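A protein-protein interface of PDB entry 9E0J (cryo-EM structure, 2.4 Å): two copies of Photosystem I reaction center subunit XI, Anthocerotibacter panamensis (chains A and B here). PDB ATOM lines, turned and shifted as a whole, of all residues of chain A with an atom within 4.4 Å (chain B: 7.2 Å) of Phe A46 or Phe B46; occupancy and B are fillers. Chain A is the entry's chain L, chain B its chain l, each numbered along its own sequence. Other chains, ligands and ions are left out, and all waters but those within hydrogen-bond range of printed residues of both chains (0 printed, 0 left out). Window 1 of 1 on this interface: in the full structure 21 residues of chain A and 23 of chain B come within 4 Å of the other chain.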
ATOM      1  N   ASP A  44     -13.539  13.239 -14.738  1.00  0.00           N
ATOM      2  CA  ASP A  44     -13.624  14.622 -15.147  1.00  0.00           C
ATOM      3  C   ASP A  44     -14.052  15.444 -13.933  1.00  0.00           C
ATOM      4  O   ASP A  44     -14.779  14.921 -13.079  1.00  0.00           O
ATOM      5  CB  ASP A  44     -14.628  14.727 -16.296  1.00  0.00           C
ATOM      6  CG  ASP A  44     -14.558  16.034 -17.034  1.00  0.00           C
ATOM      7  OD1 ASP A  44     -15.517  16.826 -16.946  1.00  0.00           O
ATOM      8  OD2 ASP A  44     -13.525  16.271 -17.692  1.00  0.00           O
ATOM      9  N   PRO A  45     -13.582  16.714 -13.796  1.00  0.00           N
ATOM     10  CA  PRO A  45     -13.960  17.569 -12.656  1.00  0.00           C
ATOM     11  C   PRO A  45     -15.448  17.816 -12.449  1.00  0.00           C
ATOM     12  O   PRO A  45     -15.888  18.063 -11.320  1.00  0.00           O
ATOM     13  CB  PRO A  45     -13.283  18.896 -12.992  1.00  0.00           C
ATOM     14  CG  PRO A  45     -12.278  18.612 -13.981  1.00  0.00           C
ATOM     15  CD  PRO A  45     -12.498  17.314 -14.592  1.00  0.00           C
ATOM     16  N   PHE A  46     -16.204  17.775 -13.548  1.00  0.00           N
ATOM     17  CA  PHE A  46     -17.652  17.931 -13.496  1.00  0.00           C
ATOM     18  C   PHE A  46     -18.323  16.813 -12.703  1.00  0.00           C
ATOM     19  O   PHE A  46     -19.171  17.087 -11.845  1.00  0.00           O
ATOM     20  CB  PHE A  46     -18.200  18.012 -14.921  1.00  0.00           C
ATOM     21  CG  PHE A  46     -19.656  17.704 -15.031  1.00  0.00           C
ATOM     22  CD1 PHE A  46     -20.086  16.491 -15.576  1.00  0.00           C
ATOM     23  CD2 PHE A  46     -20.600  18.599 -14.550  1.00  0.00           C
ATOM     24  CE1 PHE A  46     -21.424  16.199 -15.660  1.00  0.00           C
ATOM     25  CE2 PHE A  46     -21.939  18.303 -14.627  1.00  0.00           C
ATOM     26  CZ  PHE A  46     -22.345  17.109 -15.194  1.00  0.00           C
ATOM     27  N   PHE A  47     -17.932  15.554 -12.955  1.00  0.00           N
ATOM     28  CA  PHE A  47     -18.503  14.428 -12.217  1.00  0.00           C
ATOM     29  C   PHE A  47     -18.050  14.461 -10.763  1.00  0.00           C
ATOM     30  O   PHE A  47     -18.803  14.049  -9.865  1.00  0.00           O
ATOM     31  CB  PHE A  47     -18.154  13.101 -12.941  1.00  0.00           C
ATOM     32  CG  PHE A  47     -18.673  11.827 -12.259  1.00  0.00           C
ATOM     33  CD1 PHE A  47     -18.035  11.211 -11.162  1.00  0.00           C
ATOM     34  CD2 PHE A  47     -19.893  11.315 -12.666  1.00  0.00           C
ATOM     35  CE1 PHE A  47     -18.566  10.113 -10.554  1.00  0.00           C
ATOM     36  CE2 PHE A  47     -20.430  10.204 -12.049  1.00  0.00           C
ATOM     37  CZ  PHE A  47     -19.759   9.620 -10.992  1.00  0.00           C
ATOM     38  N   ARG A  48     -16.818  14.920 -10.533  1.00  0.00           N
ATOM     39  CA  ARG A  48     -16.271  15.051  -9.191  1.00  0.00           C
ATOM     40  C   ARG A  48     -17.076  16.040  -8.360  1.00  0.00           C
ATOM     41  O   ARG A  48     -17.496  15.723  -7.237  1.00  0.00           O
ATOM     42  CB  ARG A  48     -14.825  15.514  -9.285  1.00  0.00           C
ATOM     43  CG  ARG A  48     -13.858  14.527  -9.849  1.00  0.00           C
ATOM     44  CD  ARG A  48     -12.490  15.173  -9.928  1.00  0.00           C
ATOM     45  NE  ARG A  48     -11.553  14.517 -10.829  1.00  0.00           N
ATOM     46  CZ  ARG A  48     -10.866  13.425 -10.522  1.00  0.00           C
ATOM     47  NH1 ARG A  48     -10.933  12.883  -9.318  1.00  0.00           N
ATOM     48  NH2 ARG A  48     -10.084  12.869 -11.443  1.00  0.00           N
ATOM     49  N   GLY A  49     -17.346  17.216  -8.938  1.00  0.00           N
ATOM     50  CA  GLY A  49     -18.184  18.203  -8.283  1.00  0.00           C
ATOM     51  C   GLY A  49     -19.612  17.736  -8.111  1.00  0.00           C
ATOM     52  O   GLY A  49     -20.231  18.019  -7.093  1.00  0.00           O
ATOM     53  N   LEU A  50     -20.115  16.950  -9.071  1.00  0.00           N
ATOM     54  CA  LEU A  50     -21.468  16.406  -9.006  1.00  0.00           C
ATOM     55  C   LEU A  50     -21.662  15.437  -7.847  1.00  0.00           C
ATOM     56  O   LEU A  50     -22.651  15.529  -7.107  1.00  0.00           O
ATOM     57  CB  LEU A  50     -21.788  15.734 -10.328  1.00  0.00           C
ATOM     58  CG  LEU A  50     -23.106  14.997 -10.389  1.00  0.00           C
ATOM     59  CD1 LEU A  50     -24.258  15.947 -10.622  1.00  0.00           C
ATOM     60  CD2 LEU A  50     -22.956  14.032 -11.479  1.00  0.00           C
ATOM     61  N   ARG A 124     -16.072  23.566 -14.213  1.00  0.00           N
ATOM     62  CA  ARG A 124     -16.783  22.285 -14.334  1.00  0.00           C
ATOM     63  C   ARG A 124     -17.152  21.713 -12.972  1.00  0.00           C
ATOM     64  O   ARG A 124     -18.265  21.196 -12.789  1.00  0.00           O
ATOM     65  CB  ARG A 124     -15.955  21.241 -15.092  1.00  0.00           C
ATOM     66  CG  ARG A 124     -15.744  21.506 -16.555  1.00  0.00           C
ATOM     67  CD  ARG A 124     -15.098  20.326 -17.291  1.00  0.00           C
ATOM     68  NE  ARG A 124     -13.743  19.984 -16.869  1.00  0.00           N
ATOM     69  CZ  ARG A 124     -12.643  20.521 -17.378  1.00  0.00           C
ATOM     70  NH1 ARG A 124     -12.699  21.485 -18.280  1.00  0.00           N
ATOM     71  NH2 ARG A 124     -11.456  20.073 -16.978  1.00  0.00           N
ATOM     72  N   PHE A 125     -16.221  21.805 -12.014  1.00  0.00           N
ATOM     73  CA  PHE A 125     -16.482  21.413 -10.630  1.00  0.00           C
ATOM     74  C   PHE A 125     -17.595  22.236  -9.993  1.00  0.00           C
ATOM     75  O   PHE A 125     -18.449  21.676  -9.303  1.00  0.00           O
ATOM     76  CB  PHE A 125     -15.202  21.531  -9.802  1.00  0.00           C
ATOM     77  CG  PHE A 125     -15.198  20.674  -8.573  1.00  0.00           C
ATOM     78  CD1 PHE A 125     -15.726  21.152  -7.372  1.00  0.00           C
ATOM     79  CD2 PHE A 125     -14.690  19.391  -8.611  1.00  0.00           C
ATOM     80  CE1 PHE A 125     -15.739  20.364  -6.241  1.00  0.00           C
ATOM     81  CE2 PHE A 125     -14.705  18.602  -7.485  1.00  0.00           C
ATOM     82  CZ  PHE A 125     -15.224  19.084  -6.302  1.00  0.00           C
ATOM     83  N   GLY A 128     -20.979  21.136 -11.617  1.00  0.00           N
ATOM     84  CA  GLY A 128     -21.384  19.854 -11.073  1.00  0.00           C
ATOM     85  C   GLY A 128     -21.820  19.940  -9.626  1.00  0.00           C
ATOM     86  O   GLY A 128     -22.824  19.332  -9.255  1.00  0.00           O
ATOM     87  N   LEU B  43     -20.880  16.072 -30.527  1.00  0.00           N
ATOM     88  CA  LEU B  43     -21.411  16.153 -29.175  1.00  0.00           C
ATOM     89  C   LEU B  43     -20.319  15.804 -28.170  1.00  0.00           C
ATOM     90  O   LEU B  43     -19.613  14.805 -28.333  1.00  0.00           O
ATOM     91  CB  LEU B  43     -22.608  15.218 -29.008  1.00  0.00           C
ATOM     92  CG  LEU B  43     -23.904  15.518 -29.762  1.00  0.00           C
ATOM     93  CD1 LEU B  43     -25.016  14.615 -29.255  1.00  0.00           C
ATOM     94  CD2 LEU B  43     -24.301  16.977 -29.651  1.00  0.00           C
ATOM     95  N   ASP B  44     -20.163  16.654 -27.161  1.00  0.00           N
ATOM     96  CA  ASP B  44     -19.390  16.308 -25.975  1.00  0.00           C
ATOM     97  C   ASP B  44     -20.097  15.166 -25.243  1.00  0.00           C
ATOM     98  O   ASP B  44     -21.330  15.145 -25.218  1.00  0.00           O
ATOM     99  CB  ASP B  44     -19.277  17.553 -25.084  1.00  0.00           C
ATOM    100  CG  ASP B  44     -18.340  17.390 -23.906  1.00  0.00           C
ATOM    101  OD1 ASP B  44     -18.796  16.915 -22.844  1.00  0.00           O
ATOM    102  OD2 ASP B  44     -17.143  17.713 -24.045  1.00  0.00           O
ATOM    103  N   PRO B  45     -19.327  14.181 -24.638  1.00  0.00           N
ATOM    104  CA  PRO B  45     -19.947  13.024 -23.953  1.00  0.00           C
ATOM    105  C   PRO B  45     -20.932  13.314 -22.826  1.00  0.00           C
ATOM    106  O   PRO B  45     -21.815  12.490 -22.553  1.00  0.00           O
ATOM    107  CB  PRO B  45     -18.743  12.260 -23.387  1.00  0.00           C
ATOM    108  CG  PRO B  45     -17.546  12.855 -23.943  1.00  0.00           C
ATOM    109  CD  PRO B  45     -17.854  14.077 -24.683  1.00  0.00           C
ATOM    110  N   PHE B  46     -20.787  14.484 -22.198  1.00  0.00           N
ATOM    111  CA  PHE B  46     -21.741  14.943 -21.196  1.00  0.00           C
ATOM    112  C   PHE B  46     -23.128  15.158 -21.800  1.00  0.00           C
ATOM    113  O   PHE B  46     -24.133  14.774 -21.193  1.00  0.00           O
ATOM    114  CB  PHE B  46     -21.213  16.226 -20.544  1.00  0.00           C
ATOM    115  CG  PHE B  46     -22.285  17.138 -20.013  1.00  0.00           C
ATOM    116  CD1 PHE B  46     -23.002  16.812 -18.858  1.00  0.00           C
ATOM    117  CD2 PHE B  46     -22.573  18.330 -20.672  1.00  0.00           C
ATOM    118  CE1 PHE B  46     -23.987  17.652 -18.390  1.00  0.00           C
ATOM    119  CE2 PHE B  46     -23.557  19.170 -20.208  1.00  0.00           C
ATOM    120  CZ  PHE B  46     -24.261  18.832 -19.068  1.00  0.00           C
ATOM    121  N   PHE B  47     -23.200  15.755 -22.998  1.00  0.00           N
ATOM    122  CA  PHE B  47     -24.501  16.008 -23.615  1.00  0.00           C
ATOM    123  C   PHE B  47     -25.147  14.713 -24.094  1.00  0.00           C
ATOM    124  O   PHE B  47     -26.382  14.577 -24.030  1.00  0.00           O
ATOM    125  CB  PHE B  47     -24.374  17.019 -24.765  1.00  0.00           C
ATOM    126  CG  PHE B  47     -25.700  17.393 -25.382  1.00  0.00           C
ATOM    127  CD1 PHE B  47     -26.431  18.440 -24.844  1.00  0.00           C
ATOM    128  CD2 PHE B  47     -26.199  16.736 -26.515  1.00  0.00           C
ATOM    129  CE1 PHE B  47     -27.650  18.788 -25.378  1.00  0.00           C
ATOM    130  CE2 PHE B  47     -27.412  17.074 -27.043  1.00  0.00           C
ATOM    131  CZ  PHE B  47     -28.130  18.100 -26.475  1.00  0.00           C
ATOM    132  N   ARG B  48     -24.333  13.784 -24.614  1.00  0.00           N
ATOM    133  CA  ARG B  48     -24.823  12.467 -25.009  1.00  0.00           C
ATOM    134  C   ARG B  48     -25.397  11.719 -23.819  1.00  0.00           C
ATOM    135  O   ARG B  48     -26.503  11.178 -23.915  1.00  0.00           O
ATOM    136  CB  ARG B  48     -23.707  11.641 -25.646  1.00  0.00           C
ATOM    137  CG  ARG B  48     -22.703  12.428 -26.441  1.00  0.00           C
ATOM    138  CD  ARG B  48     -21.645  11.510 -27.003  1.00  0.00           C
ATOM    139  NE  ARG B  48     -20.799  12.153 -27.999  1.00  0.00           N
ATOM    140  CZ  ARG B  48     -20.998  12.085 -29.306  1.00  0.00           C
ATOM    141  NH1 ARG B  48     -22.014  11.412 -29.815  1.00  0.00           N
ATOM    142  NH2 ARG B  48     -20.170  12.729 -30.123  1.00  0.00           N
ATOM    143  N   GLY B  49     -24.683  11.752 -22.682  1.00  0.00           N
ATOM    144  CA  GLY B  49     -25.199  11.172 -21.452  1.00  0.00           C
ATOM    145  C   GLY B  49     -26.468  11.837 -20.960  1.00  0.00           C
ATOM    146  O   GLY B  49     -27.394  11.150 -20.541  1.00  0.00           O
ATOM    147  N   LEU B  50     -26.553  13.170 -21.101  1.00  0.00           N
ATOM    148  CA  LEU B  50     -27.729  13.939 -20.686  1.00  0.00           C
ATOM    149  C   LEU B  50     -28.974  13.558 -21.469  1.00  0.00           C
ATOM    150  O   LEU B  50     -30.053  13.353 -20.894  1.00  0.00           O
ATOM    151  CB  LEU B  50     -27.448  15.424 -20.857  1.00  0.00           C
ATOM    152  CG  LEU B  50     -28.574  16.388 -20.505  1.00  0.00           C
ATOM    153  CD1 LEU B  50     -29.017  16.239 -19.089  1.00  0.00           C
ATOM    154  CD2 LEU B  50     -28.104  17.741 -20.708  1.00  0.00           C
ATOM    155  N   GLU B  51     -28.821  13.393 -22.771  1.00  0.00           N
ATOM    156  CA  GLU B  51     -29.963  13.098 -23.615  1.00  0.00           C
ATOM    157  C   GLU B  51     -30.423  11.640 -23.462  1.00  0.00           C
ATOM    158  O   GLU B  51     -31.642  11.374 -23.374  1.00  0.00           O
ATOM    159  CB  GLU B  51     -29.558  13.413 -25.036  1.00  0.00           C
ATOM    160  CG  GLU B  51     -30.454  12.908 -26.019  1.00  0.00           C
ATOM    161  CD  GLU B  51     -30.323  13.626 -27.300  1.00  0.00           C
ATOM    162  OE1 GLU B  51     -29.307  14.299 -27.548  1.00  0.00           O
ATOM    163  OE2 GLU B  51     -31.130  13.317 -28.151  1.00  0.00           O
ATOM    164  N   VAL B  52     -29.457  10.695 -23.402  1.00  0.00           N
ATOM    165  CA  VAL B  52     -29.725   9.292 -23.042  1.00  0.00           C
ATOM    166  C   VAL B  52     -30.412   9.178 -21.686  1.00  0.00           C
ATOM    167  O   VAL B  52     -31.389   8.422 -21.535  1.00  0.00           O
ATOM    168  CB  VAL B  52     -28.420   8.464 -23.105  1.00  0.00           C
ATOM    169  CG1 VAL B  52     -28.644   7.034 -22.746  1.00  0.00           C
ATOM    170  CG2 VAL B  52     -27.965   8.367 -24.549  1.00  0.00           C
ATOM    171  N   PHE B 117     -13.835   8.136 -25.974  1.00  0.00           N
ATOM    172  CA  PHE B 117     -13.971   8.748 -24.673  1.00  0.00           C
ATOM    173  C   PHE B 117     -12.799   8.208 -23.884  1.00  0.00           C
ATOM    174  O   PHE B 117     -12.379   7.067 -24.091  1.00  0.00           O
ATOM    175  CB  PHE B 117     -15.249   8.316 -23.952  1.00  0.00           C
ATOM    176  CG  PHE B 117     -16.524   8.774 -24.590  1.00  0.00           C
ATOM    177  CD1 PHE B 117     -16.559   9.763 -25.576  1.00  0.00           C
ATOM    178  CD2 PHE B 117     -17.712   8.188 -24.190  1.00  0.00           C
ATOM    179  CE1 PHE B 117     -17.741  10.104 -26.177  1.00  0.00           C
ATOM    180  CE2 PHE B 117     -18.894   8.559 -24.755  1.00  0.00           C
ATOM    181  CZ  PHE B 117     -18.913   9.516 -25.751  1.00  0.00           C
ATOM    182  N   GLU B 120     -12.372   9.989 -18.403  1.00  0.00           N
ATOM    183  CA  GLU B 120     -12.980  11.277 -18.102  1.00  0.00           C
ATOM    184  C   GLU B 120     -14.207  11.515 -18.972  1.00  0.00           C
ATOM    185  O   GLU B 120     -15.204  12.069 -18.499  1.00  0.00           O
ATOM    186  CB  GLU B 120     -11.975  12.435 -18.281  1.00  0.00           C
ATOM    187  CG  GLU B 120     -10.549  12.453 -17.573  1.00  0.00           C
ATOM    188  CD  GLU B 120      -9.606  11.265 -17.828  1.00  0.00           C
ATOM    189  OE1 GLU B 120      -8.938  10.811 -16.874  1.00  0.00           O
ATOM    190  OE2 GLU B 120      -9.557  10.776 -18.978  1.00  0.00           O
ATOM    191  N   GLY B 121     -14.162  11.075 -20.235  1.00  0.00           N
ATOM    192  CA  GLY B 121     -15.326  11.187 -21.103  1.00  0.00           C
ATOM    193  C   GLY B 121     -16.478  10.294 -20.676  1.00  0.00           C
ATOM    194  O   GLY B 121     -17.641  10.706 -20.708  1.00  0.00           O
ATOM    195  N   SER B 123     -16.917   9.452 -17.574  1.00  0.00           N
ATOM    196  CA  SER B 123     -17.416  10.067 -16.345  1.00  0.00           C
ATOM    197  C   SER B 123     -18.311  11.273 -16.637  1.00  0.00           C
ATOM    198  O   SER B 123     -19.282  11.518 -15.908  1.00  0.00           O
ATOM    199  CB  SER B 123     -16.245  10.443 -15.435  1.00  0.00           C
ATOM    200  OG  SER B 123     -15.588  11.604 -15.887  1.00  0.00           O
ATOM    201  N   ARG B 124     -18.007  12.019 -17.711  1.00  0.00           N
ATOM    202  CA  ARG B 124     -18.909  13.065 -18.209  1.00  0.00           C
ATOM    203  C   ARG B 124     -20.243  12.489 -18.657  1.00  0.00           C
ATOM    204  O   ARG B 124     -21.302  13.070 -18.381  1.00  0.00           O
ATOM    205  CB  ARG B 124     -18.279  13.813 -19.383  1.00  0.00           C
ATOM    206  CG  ARG B 124     -17.112  14.671 -19.030  1.00  0.00           C
ATOM    207  CD  ARG B 124     -16.940  15.882 -19.959  1.00  0.00           C
ATOM    208  NE  ARG B 124     -16.311  15.647 -21.266  1.00  0.00           N
ATOM    209  CZ  ARG B 124     -15.091  15.173 -21.525  1.00  0.00           C
ATOM    210  NH1 ARG B 124     -14.195  14.960 -20.572  1.00  0.00           N
ATOM    211  NH2 ARG B 124     -14.742  14.953 -22.790  1.00  0.00           N
ATOM    212  N   PHE B 125     -20.195  11.344 -19.354  1.00  0.00           N
ATOM    213  CA  PHE B 125     -21.404  10.624 -19.748  1.00  0.00           C
ATOM    214  C   PHE B 125     -22.190  10.146 -18.530  1.00  0.00           C
ATOM    215  O   PHE B 125     -23.418  10.236 -18.526  1.00  0.00           O
ATOM    216  CB  PHE B 125     -21.023   9.474 -20.707  1.00  0.00           C
ATOM    217  CG  PHE B 125     -22.199   8.818 -21.444  1.00  0.00           C
ATOM    218  CD1 PHE B 125     -23.092   7.927 -20.822  1.00  0.00           C
ATOM    219  CD2 PHE B 125     -22.461   9.187 -22.753  1.00  0.00           C
ATOM    220  CE1 PHE B 125     -24.161   7.385 -21.513  1.00  0.00           C
ATOM    221  CE2 PHE B 125     -23.547   8.660 -23.433  1.00  0.00           C
ATOM    222  CZ  PHE B 125     -24.384   7.756 -22.817  1.00  0.00           C
ATOM    223  N   ALA B 126     -21.497   9.639 -17.503  1.00  0.00           N
ATOM    224  CA  ALA B 126     -22.137   9.189 -16.265  1.00  0.00           C
ATOM    225  C   ALA B 126     -22.837  10.331 -15.539  1.00  0.00           C
ATOM    226  O   ALA B 126     -23.975  10.174 -15.069  1.00  0.00           O
ATOM    227  CB  ALA B 126     -21.092   8.557 -15.351  1.00  0.00           C
ATOM    228  N   GLY B 127     -22.179  11.493 -15.486  1.00  0.00           N
ATOM    229  CA  GLY B 127     -22.772  12.661 -14.856  1.00  0.00           C
ATOM    230  C   GLY B 127     -23.980  13.198 -15.599  1.00  0.00           C
ATOM    231  O   GLY B 127     -25.014  13.513 -14.985  1.00  0.00           O
ATOM    232  N   GLY B 128     -23.868  13.281 -16.933  1.00  0.00           N
ATOM    233  CA  GLY B 128     -25.002  13.653 -17.761  1.00  0.00           C
ATOM    234  C   GLY B 128     -26.148  12.668 -17.667  1.00  0.00           C
ATOM    235  O   GLY B 128     -27.304  13.079 -17.590  1.00  0.00           O
ATOM    236  N   TRP B 129     -25.826  11.365 -17.584  1.00  0.00           N
ATOM    237  CA  TRP B 129     -26.819  10.304 -17.436  1.00  0.00           C
ATOM    238  C   TRP B 129     -27.608  10.444 -16.151  1.00  0.00           C
ATOM    239  O   TRP B 129     -28.833  10.315 -16.161  1.00  0.00           O
ATOM    240  CB  TRP B 129     -26.133   8.934 -17.486  1.00  0.00           C
ATOM    241  CG  TRP B 129     -26.931   7.836 -16.814  1.00  0.00           C
ATOM    242  CD1 TRP B 129     -26.760   7.337 -15.551  1.00  0.00           C
ATOM    243  CD2 TRP B 129     -28.012   7.106 -17.381  1.00  0.00           C
ATOM    244  NE1 TRP B 129     -27.687   6.365 -15.294  1.00  0.00           N
ATOM    245  CE2 TRP B 129     -28.465   6.197 -16.405  1.00  0.00           C
ATOM    246  CE3 TRP B 129     -28.637   7.124 -18.625  1.00  0.00           C
ATOM    247  CZ2 TRP B 129     -29.521   5.322 -16.635  1.00  0.00           C
ATOM    248  CZ3 TRP B 129     -29.678   6.278 -18.849  1.00  0.00           C
ATOM    249  CH2 TRP B 129     -30.125   5.387 -17.856  1.00  0.00           C
ATOM    250  N   ILE B 131     -28.010  13.278 -14.227  1.00  0.00           N
ATOM    251  CA  ILE B 131     -28.813  14.501 -14.217  1.00  0.00           C
ATOM    252  C   ILE B 131     -30.001  14.390 -15.162  1.00  0.00           C
ATOM    253  O   ILE B 131     -31.138  14.705 -14.780  1.00  0.00           O
ATOM    254  CB  ILE B 131     -27.947  15.723 -14.549  1.00  0.00           C
ATOM    255  CG1 ILE B 131     -26.840  15.876 -13.521  1.00  0.00           C
ATOM    256  CG2 ILE B 131     -28.776  16.962 -14.604  1.00  0.00           C
ATOM    257  CD1 ILE B 131     -25.704  16.632 -14.044  1.00  0.00           C
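Asp A44 touches Glu B120. Phe A46 touches Phe B46 (CE1 to CD1, 3.6 Å). CA of Gly B127 touches CE1 of Phe A46 (3.9 Å). CZ of Phe A46 touches CD1 of Ile B131, at 3.6 Å. Phe A47 touches Ser B123 (CD2 to O, 3.3 Å). Ala B126 touches Phe A47 (CB to CE2, 3.7 Å). Phe A47 touches Gly B127 (CD2 to N, 3.6 Å). Leu A50 touches Gly B127 (CD2 to CA, 3.6 Å). CD1 of Leu A50 touches CD1 of Ile B131 (3.8 Å).
N of Phe B46 sits close to OD1 of Asp B44, at 3.2 Å. The guanidinium group (NE) of Arg B124 lies within salt-bridge range of the side-chain carboxylate (OD1) of Asp B44 (3.2 Å). The backbone carbonyl oxygen (O) of Glu B120 lies within hydrogen-bond range of the side-chain hydroxyl (OG) of Ser B123 (2.7 Å). The guanidinium group (NE) of Arg A124 lies within salt-bridge range of the side-chain carboxylate (OD1) of Asp A44 (3.6 Å).
The backbone NH (N) of Asp A44 is in hydrogen-bond range of the side-chain hydroxyl (OG) of Ser B123, at 2.9 Å. NH1 of Arg B124 is in salt-bridge range of OD2 of Asp A44 (3.2 Å).
Asp A44 touches Arg B124, but with the chains exchanged Arg A124 does not touch Asp B44 (7.5 Å). Phe B46 touches its own counterpart, Phe A46. Positions printed for both chains: 44, 45, 46, 47, 48, 49, 50, 124, 125 and 128.
Of the printed residues of chain B, Phe A46 touches Phe B46 (3.6 Å), Gly B127 (3.9 Å) and Ile B131 (3.6 Å). Printed residues of chain B within 4 Å of Leu A50: Gly B127 and Ile B131. Phe B46 touches just one residue of chain A: Phe A46. Of the printed residues of chain A, Glu B120 touches Asp A44. Of the printed residues of chain A, Arg B124 touches Asp A44. Of the printed residues of chain A, Ala B126 touches Phe A47. The nearest printed residue of chain B that does not touch Phe A46 is Gly B128 (4.01 Å).
Hydrophobic or aromatic side chains of chain B that line the printed part of chain A: Phe B46, Ala B126 and Ile B131. Of the 10 printed residues of chain A, 4 touch a printed residue of chain B. Hydrophobic or aromatic side chains of chain A that line the printed part of chain B: Phe A46, Phe A47 and Leu A50. Among the printed residues, 11 pairs touch across the chains. Among the printed residues, Asp or Glu carboxylates within 4 Å of a Lys or Arg side-chain nitrogen of the other chain: Asp A44 with Arg B124 (3.2 Å).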
